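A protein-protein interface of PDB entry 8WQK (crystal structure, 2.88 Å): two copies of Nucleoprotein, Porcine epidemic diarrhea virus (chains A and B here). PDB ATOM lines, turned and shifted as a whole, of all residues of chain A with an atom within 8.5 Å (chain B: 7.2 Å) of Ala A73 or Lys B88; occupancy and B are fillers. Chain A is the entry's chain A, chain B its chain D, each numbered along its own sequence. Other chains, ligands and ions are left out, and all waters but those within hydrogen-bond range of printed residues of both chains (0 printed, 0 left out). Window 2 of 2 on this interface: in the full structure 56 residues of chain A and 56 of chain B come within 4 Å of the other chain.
OG of Ser A75 is in hydrogen-bond range of OD1 of Asp A74.
OE2 of Glu A71 is in salt-bridge range of NZ of Lys B88 (3.0 Å).
NZ of Lys B88 sits at hydrogen-bond distance from O of Leu A72 (3.0 Å).
The side-chain amino group (NZ) of Lys B88 lies within hydrogen-bond range of the backbone carbonyl oxygen (O) of Ala A73.
N of Lys B88 is in hydrogen-bond range of O of Asp A74.
The backbone carbonyl oxygen (O) of Tyr A76 sits at hydrogen-bond distance from the backbone NH (N) of Val B86, at 2.8 Å.
OH of Tyr A76 is in hydrogen-bond range of OE2 of Glu B94 (3.2 Å).
Of chain B, only Lys B88 comes within 4 Å of Ala A73.
Lys B88 touches six residues of chain A.
No residue of chain A comes within 4 Å of Ser B89.
Printed residues of chain B within 4 Å of Tyr A76: Val B86, Lys B88, Val B93 and Glu B94.
Of the printed residues of chain B, Glu A71 touches Lys B88 (3.0 Å).
No position is printed for both chains.
Pro B87 touches Asp A74 (CA to O, 3.9 Å).
CB of Ser A75 touches O of Val B86 (3.2 Å).
Ser A75 touches Lys B88.
CE2 of Tyr A76 touches CG of Lys B88, 3.5 Å away.
CD2 of Tyr A76 touches CG1 of Val B93, at 3.6 Å.
Printed residues of chain B that touch a printed residue of chain A: Val B86, Pro B87, Lys B88, Val B93 and Glu B94.
Hydrophobic or aromatic side chains of chain B that line the printed part of chain A: Val B86 and Val B93.
Along chain B the printed residues that touch a printed residue of chain A span positions 86 to 94.
Hydrophobic or aromatic side chains of chain A that line the printed part of chain B: Tyr A76.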
ATOM      1  N   ARG A  70       5.680 -13.143 -17.378  1.00  0.00           N
ATOM      2  CA  ARG A  70       5.191 -11.995 -16.625  1.00  0.00           C
ATOM      3  C   ARG A  70       6.076 -11.883 -15.392  1.00  0.00           C
ATOM      4  O   ARG A  70       6.170 -12.832 -14.608  1.00  0.00           O
ATOM      5  CB  ARG A  70       3.715 -12.183 -16.251  1.00  0.00           C
ATOM      6  CG  ARG A  70       2.891 -10.914 -16.069  1.00  0.00           C
ATOM      7  CD  ARG A  70       1.366 -11.177 -15.952  1.00  0.00           C
ATOM      8  NE  ARG A  70       1.019 -12.221 -14.996  1.00  0.00           N
ATOM      9  CZ  ARG A  70       0.786 -12.033 -13.699  1.00  0.00           C
ATOM     10  NH1 ARG A  70       0.594 -10.828 -13.193  1.00  0.00           N
ATOM     11  NH2 ARG A  70       0.667 -13.091 -12.904  1.00  0.00           N
ATOM     12  N   GLU A  71       6.747 -10.751 -15.226  1.00  0.00           N
ATOM     13  CA  GLU A  71       7.617 -10.588 -14.068  1.00  0.00           C
ATOM     14  C   GLU A  71       6.820 -10.101 -12.872  1.00  0.00           C
ATOM     15  O   GLU A  71       6.068  -9.128 -12.968  1.00  0.00           O
ATOM     16  CB  GLU A  71       8.758  -9.616 -14.318  1.00  0.00           C
ATOM     17  CG  GLU A  71       9.704  -9.585 -13.128  1.00  0.00           C
ATOM     18  CD  GLU A  71      10.830  -8.578 -13.303  1.00  0.00           C
ATOM     19  OE1 GLU A  71      10.945  -8.007 -14.421  1.00  0.00           O
ATOM     20  OE2 GLU A  71      11.588  -8.360 -12.319  1.00  0.00           O
ATOM     21  N   LEU A  72       7.021 -10.750 -11.745  1.00  0.00           N
ATOM     22  CA  LEU A  72       6.437 -10.328 -10.487  1.00  0.00           C
ATOM     23  C   LEU A  72       7.531  -9.778  -9.579  1.00  0.00           C
ATOM     24  O   LEU A  72       8.699  -9.638  -9.969  1.00  0.00           O
ATOM     25  CB  LEU A  72       5.686 -11.494  -9.840  1.00  0.00           C
ATOM     26  CG  LEU A  72       4.724 -12.248 -10.772  1.00  0.00           C
ATOM     27  CD1 LEU A  72       3.888 -13.222  -9.983  1.00  0.00           C
ATOM     28  CD2 LEU A  72       3.826 -11.297 -11.555  1.00  0.00           C
ATOM     29  N   ALA A  73       7.130  -9.427  -8.362  1.00  0.00           N
ATOM     30  CA  ALA A  73       8.086  -8.872  -7.420  1.00  0.00           C
ATOM     31  C   ALA A  73       9.153  -9.896  -7.076  1.00  0.00           C
ATOM     32  O   ALA A  73      10.353  -9.632  -7.220  1.00  0.00           O
ATOM     33  CB  ALA A  73       7.363  -8.398  -6.156  1.00  0.00           C
ATOM     34  N   ASP A  74       8.738 -11.109  -6.731  1.00  0.00           N
ATOM     35  CA  ASP A  74       9.654 -12.097  -6.185  1.00  0.00           C
ATOM     36  C   ASP A  74       9.813 -13.298  -7.093  1.00  0.00           C
ATOM     37  O   ASP A  74      10.403 -14.298  -6.677  1.00  0.00           O
ATOM     38  CB  ASP A  74       9.156 -12.593  -4.824  1.00  0.00           C
ATOM     39  CG  ASP A  74       7.757 -13.250  -4.902  1.00  0.00           C
ATOM     40  OD1 ASP A  74       7.188 -13.344  -6.013  1.00  0.00           O
ATOM     41  OD2 ASP A  74       7.223 -13.674  -3.851  1.00  0.00           O
ATOM     42  N   SER A  75       9.287 -13.234  -8.311  1.00  0.00           N
ATOM     43  CA  SER A  75       9.212 -14.438  -9.120  1.00  0.00           C
ATOM     44  C   SER A  75       8.977 -14.063 -10.575  1.00  0.00           C
ATOM     45  O   SER A  75       8.726 -12.903 -10.909  1.00  0.00           O
ATOM     46  CB  SER A  75       8.119 -15.367  -8.582  1.00  0.00           C
ATOM     47  OG  SER A  75       6.869 -14.693  -8.522  1.00  0.00           O
ATOM     48  N   TYR A  76       9.093 -15.068 -11.442  1.00  0.00           N
ATOM     49  CA  TYR A  76       8.659 -14.983 -12.830  1.00  0.00           C
ATOM     50  C   TYR A  76       7.581 -16.028 -13.042  1.00  0.00           C
ATOM     51  O   TYR A  76       7.727 -17.172 -12.598  1.00  0.00           O
ATOM     52  CB  TYR A  76       9.810 -15.247 -13.813  1.00  0.00           C
ATOM     53  CG  TYR A  76      10.844 -14.153 -13.898  1.00  0.00           C
ATOM     54  CD1 TYR A  76      10.680 -13.068 -14.752  1.00  0.00           C
ATOM     55  CD2 TYR A  76      11.993 -14.216 -13.131  1.00  0.00           C
ATOM     56  CE1 TYR A  76      11.636 -12.087 -14.829  1.00  0.00           C
ATOM     57  CE2 TYR A  76      12.936 -13.242 -13.198  1.00  0.00           C
ATOM     58  CZ  TYR A  76      12.764 -12.181 -14.045  1.00  0.00           C
ATOM     59  OH  TYR A  76      13.754 -11.220 -14.078  1.00  0.00           O
ATOM     60  N   GLU A  77       6.522 -15.653 -13.745  1.00  0.00           N
ATOM     61  CA  GLU A  77       5.462 -16.576 -14.103  1.00  0.00           C
ATOM     62  C   GLU A  77       5.595 -16.862 -15.590  1.00  0.00           C
ATOM     63  O   GLU A  77       5.472 -15.947 -16.417  1.00  0.00           O
ATOM     64  CB  GLU A  77       4.103 -15.979 -13.750  1.00  0.00           C
ATOM     65  CG  GLU A  77       3.010 -16.249 -14.757  1.00  0.00           C
ATOM     66  CD  GLU A  77       1.707 -15.551 -14.395  1.00  0.00           C
ATOM     67  OE1 GLU A  77       1.268 -15.652 -13.214  1.00  0.00           O
ATOM     68  OE2 GLU A  77       1.127 -14.897 -15.303  1.00  0.00           O
ATOM     69  N   VAL B  86       8.184 -19.534 -11.107  1.00  0.00           N
ATOM     70  CA  VAL B  86       9.555 -19.817 -10.701  1.00  0.00           C
ATOM     71  C   VAL B  86      10.025 -18.695  -9.786  1.00  0.00           C
ATOM     72  O   VAL B  86       9.904 -17.520 -10.156  1.00  0.00           O
ATOM     73  CB  VAL B  86      10.493 -19.922 -11.917  1.00  0.00           C
ATOM     74  CG1 VAL B  86      11.871 -20.345 -11.477  1.00  0.00           C
ATOM     75  CG2 VAL B  86       9.931 -20.858 -12.955  1.00  0.00           C
ATOM     76  N   PRO B  87      10.585 -19.009  -8.615  1.00  0.00           N
ATOM     77  CA  PRO B  87      11.124 -17.963  -7.740  1.00  0.00           C
ATOM     78  C   PRO B  87      12.334 -17.276  -8.354  1.00  0.00           C
ATOM     79  O   PRO B  87      13.209 -17.925  -8.928  1.00  0.00           O
ATOM     80  CB  PRO B  87      11.520 -18.737  -6.479  1.00  0.00           C
ATOM     81  CG  PRO B  87      10.646 -19.959  -6.504  1.00  0.00           C
ATOM     82  CD  PRO B  87      10.562 -20.319  -7.954  1.00  0.00           C
ATOM     83  N   LYS B  88      12.427 -15.959  -8.151  1.00  0.00           N
ATOM     84  CA  LYS B  88      13.561 -15.192  -8.675  1.00  0.00           C
ATOM     85  C   LYS B  88      14.881 -15.633  -8.059  1.00  0.00           C
ATOM     86  O   LYS B  88      15.943 -15.356  -8.623  1.00  0.00           O
ATOM     87  CB  LYS B  88      13.327 -13.697  -8.459  1.00  0.00           C
ATOM     88  CG  LYS B  88      12.825 -12.979  -9.704  1.00  0.00           C
ATOM     89  CD  LYS B  88      13.008 -11.478  -9.574  1.00  0.00           C
ATOM     90  CE  LYS B  88      11.911 -10.700 -10.275  1.00  0.00           C
ATOM     91  NZ  LYS B  88      11.630  -9.429  -9.567  1.00  0.00           N
ATOM     92  N   SER B  89      14.827 -16.343  -6.931  1.00  0.00           N
ATOM     93  CA  SER B  89      15.989 -16.958  -6.308  1.00  0.00           C
ATOM     94  C   SER B  89      16.552 -18.131  -7.112  1.00  0.00           C
ATOM     95  O   SER B  89      17.615 -18.650  -6.748  1.00  0.00           O
ATOM     96  CB  SER B  89      15.606 -17.437  -4.916  1.00  0.00           C
ATOM     97  OG  SER B  89      14.560 -18.395  -5.000  1.00  0.00           O
ATOM     98  N   ASP B  90      15.835 -18.613  -8.131  1.00  0.00           N
ATOM     99  CA  ASP B  90      16.352 -19.693  -8.967  1.00  0.00           C
ATOM    100  C   ASP B  90      17.473 -19.167  -9.859  1.00  0.00           C
ATOM    101  O   ASP B  90      17.299 -18.145 -10.541  1.00  0.00           O
ATOM    102  CB  ASP B  90      15.221 -20.288  -9.799  1.00  0.00           C
ATOM    103  CG  ASP B  90      15.608 -21.573 -10.497  1.00  0.00           C
ATOM    104  OD1 ASP B  90      16.287 -21.519 -11.555  1.00  0.00           O
ATOM    105  OD2 ASP B  90      15.213 -22.645  -9.996  1.00  0.00           O
ATOM    106  N   PRO B  91      18.615 -19.854  -9.926  1.00  0.00           N
ATOM    107  CA  PRO B  91      19.761 -19.299 -10.668  1.00  0.00           C
ATOM    108  C   PRO B  91      19.563 -19.280 -12.177  1.00  0.00           C
ATOM    109  O   PRO B  91      20.380 -18.683 -12.894  1.00  0.00           O
ATOM    110  CB  PRO B  91      20.928 -20.216 -10.270  1.00  0.00           C
ATOM    111  CG  PRO B  91      20.320 -21.393  -9.524  1.00  0.00           C
ATOM    112  CD  PRO B  91      18.836 -21.233  -9.458  1.00  0.00           C
ATOM    113  N   ASN B  92      18.515 -19.906 -12.685  1.00  0.00           N
ATOM    114  CA  ASN B  92      18.359 -20.064 -14.116  1.00  0.00           C
ATOM    115  C   ASN B  92      17.241 -19.227 -14.731  1.00  0.00           C
ATOM    116  O   ASN B  92      17.044 -19.314 -15.956  1.00  0.00           O
ATOM    117  CB  ASN B  92      18.167 -21.556 -14.438  1.00  0.00           C
ATOM    118  CG  ASN B  92      19.302 -22.423 -13.884  1.00  0.00           C
ATOM    119  OD1 ASN B  92      20.481 -22.126 -14.090  1.00  0.00           O
ATOM    120  ND2 ASN B  92      18.943 -23.489 -13.165  1.00  0.00           N
ATOM    121  N   VAL B  93      16.445 -18.505 -13.928  1.00  0.00           N
ATOM    122  CA  VAL B  93      15.273 -17.855 -14.507  1.00  0.00           C
ATOM    123  C   VAL B  93      15.675 -16.744 -15.483  1.00  0.00           C
ATOM    124  O   VAL B  93      15.087 -16.644 -16.564  1.00  0.00           O
ATOM    125  CB  VAL B  93      14.302 -17.358 -13.425  1.00  0.00           C
ATOM    126  CG1 VAL B  93      12.895 -17.651 -13.854  1.00  0.00           C
ATOM    127  CG2 VAL B  93      14.607 -18.024 -12.174  1.00  0.00           C
ATOM    128  N   GLU B  94      16.642 -15.862 -15.141  1.00  0.00           N
ATOM    129  CA  GLU B  94      17.172 -15.019 -16.239  1.00  0.00           C
ATOM    130  C   GLU B  94      17.813 -15.746 -17.376  1.00  0.00           C
ATOM    131  O   GLU B  94      17.607 -15.337 -18.524  1.00  0.00           O
ATOM    132  CB  GLU B  94      18.161 -13.936 -15.857  1.00  0.00           C
ATOM    133  CG  GLU B  94      17.734 -12.686 -15.152  1.00  0.00           C
ATOM    134  CD  GLU B  94      17.163 -11.740 -16.287  1.00  0.00           C
ATOM    135  OE1 GLU B  94      17.812 -11.836 -17.431  1.00  0.00           O
ATOM    136  OE2 GLU B  94      16.149 -11.060 -16.139  1.00  0.00           O
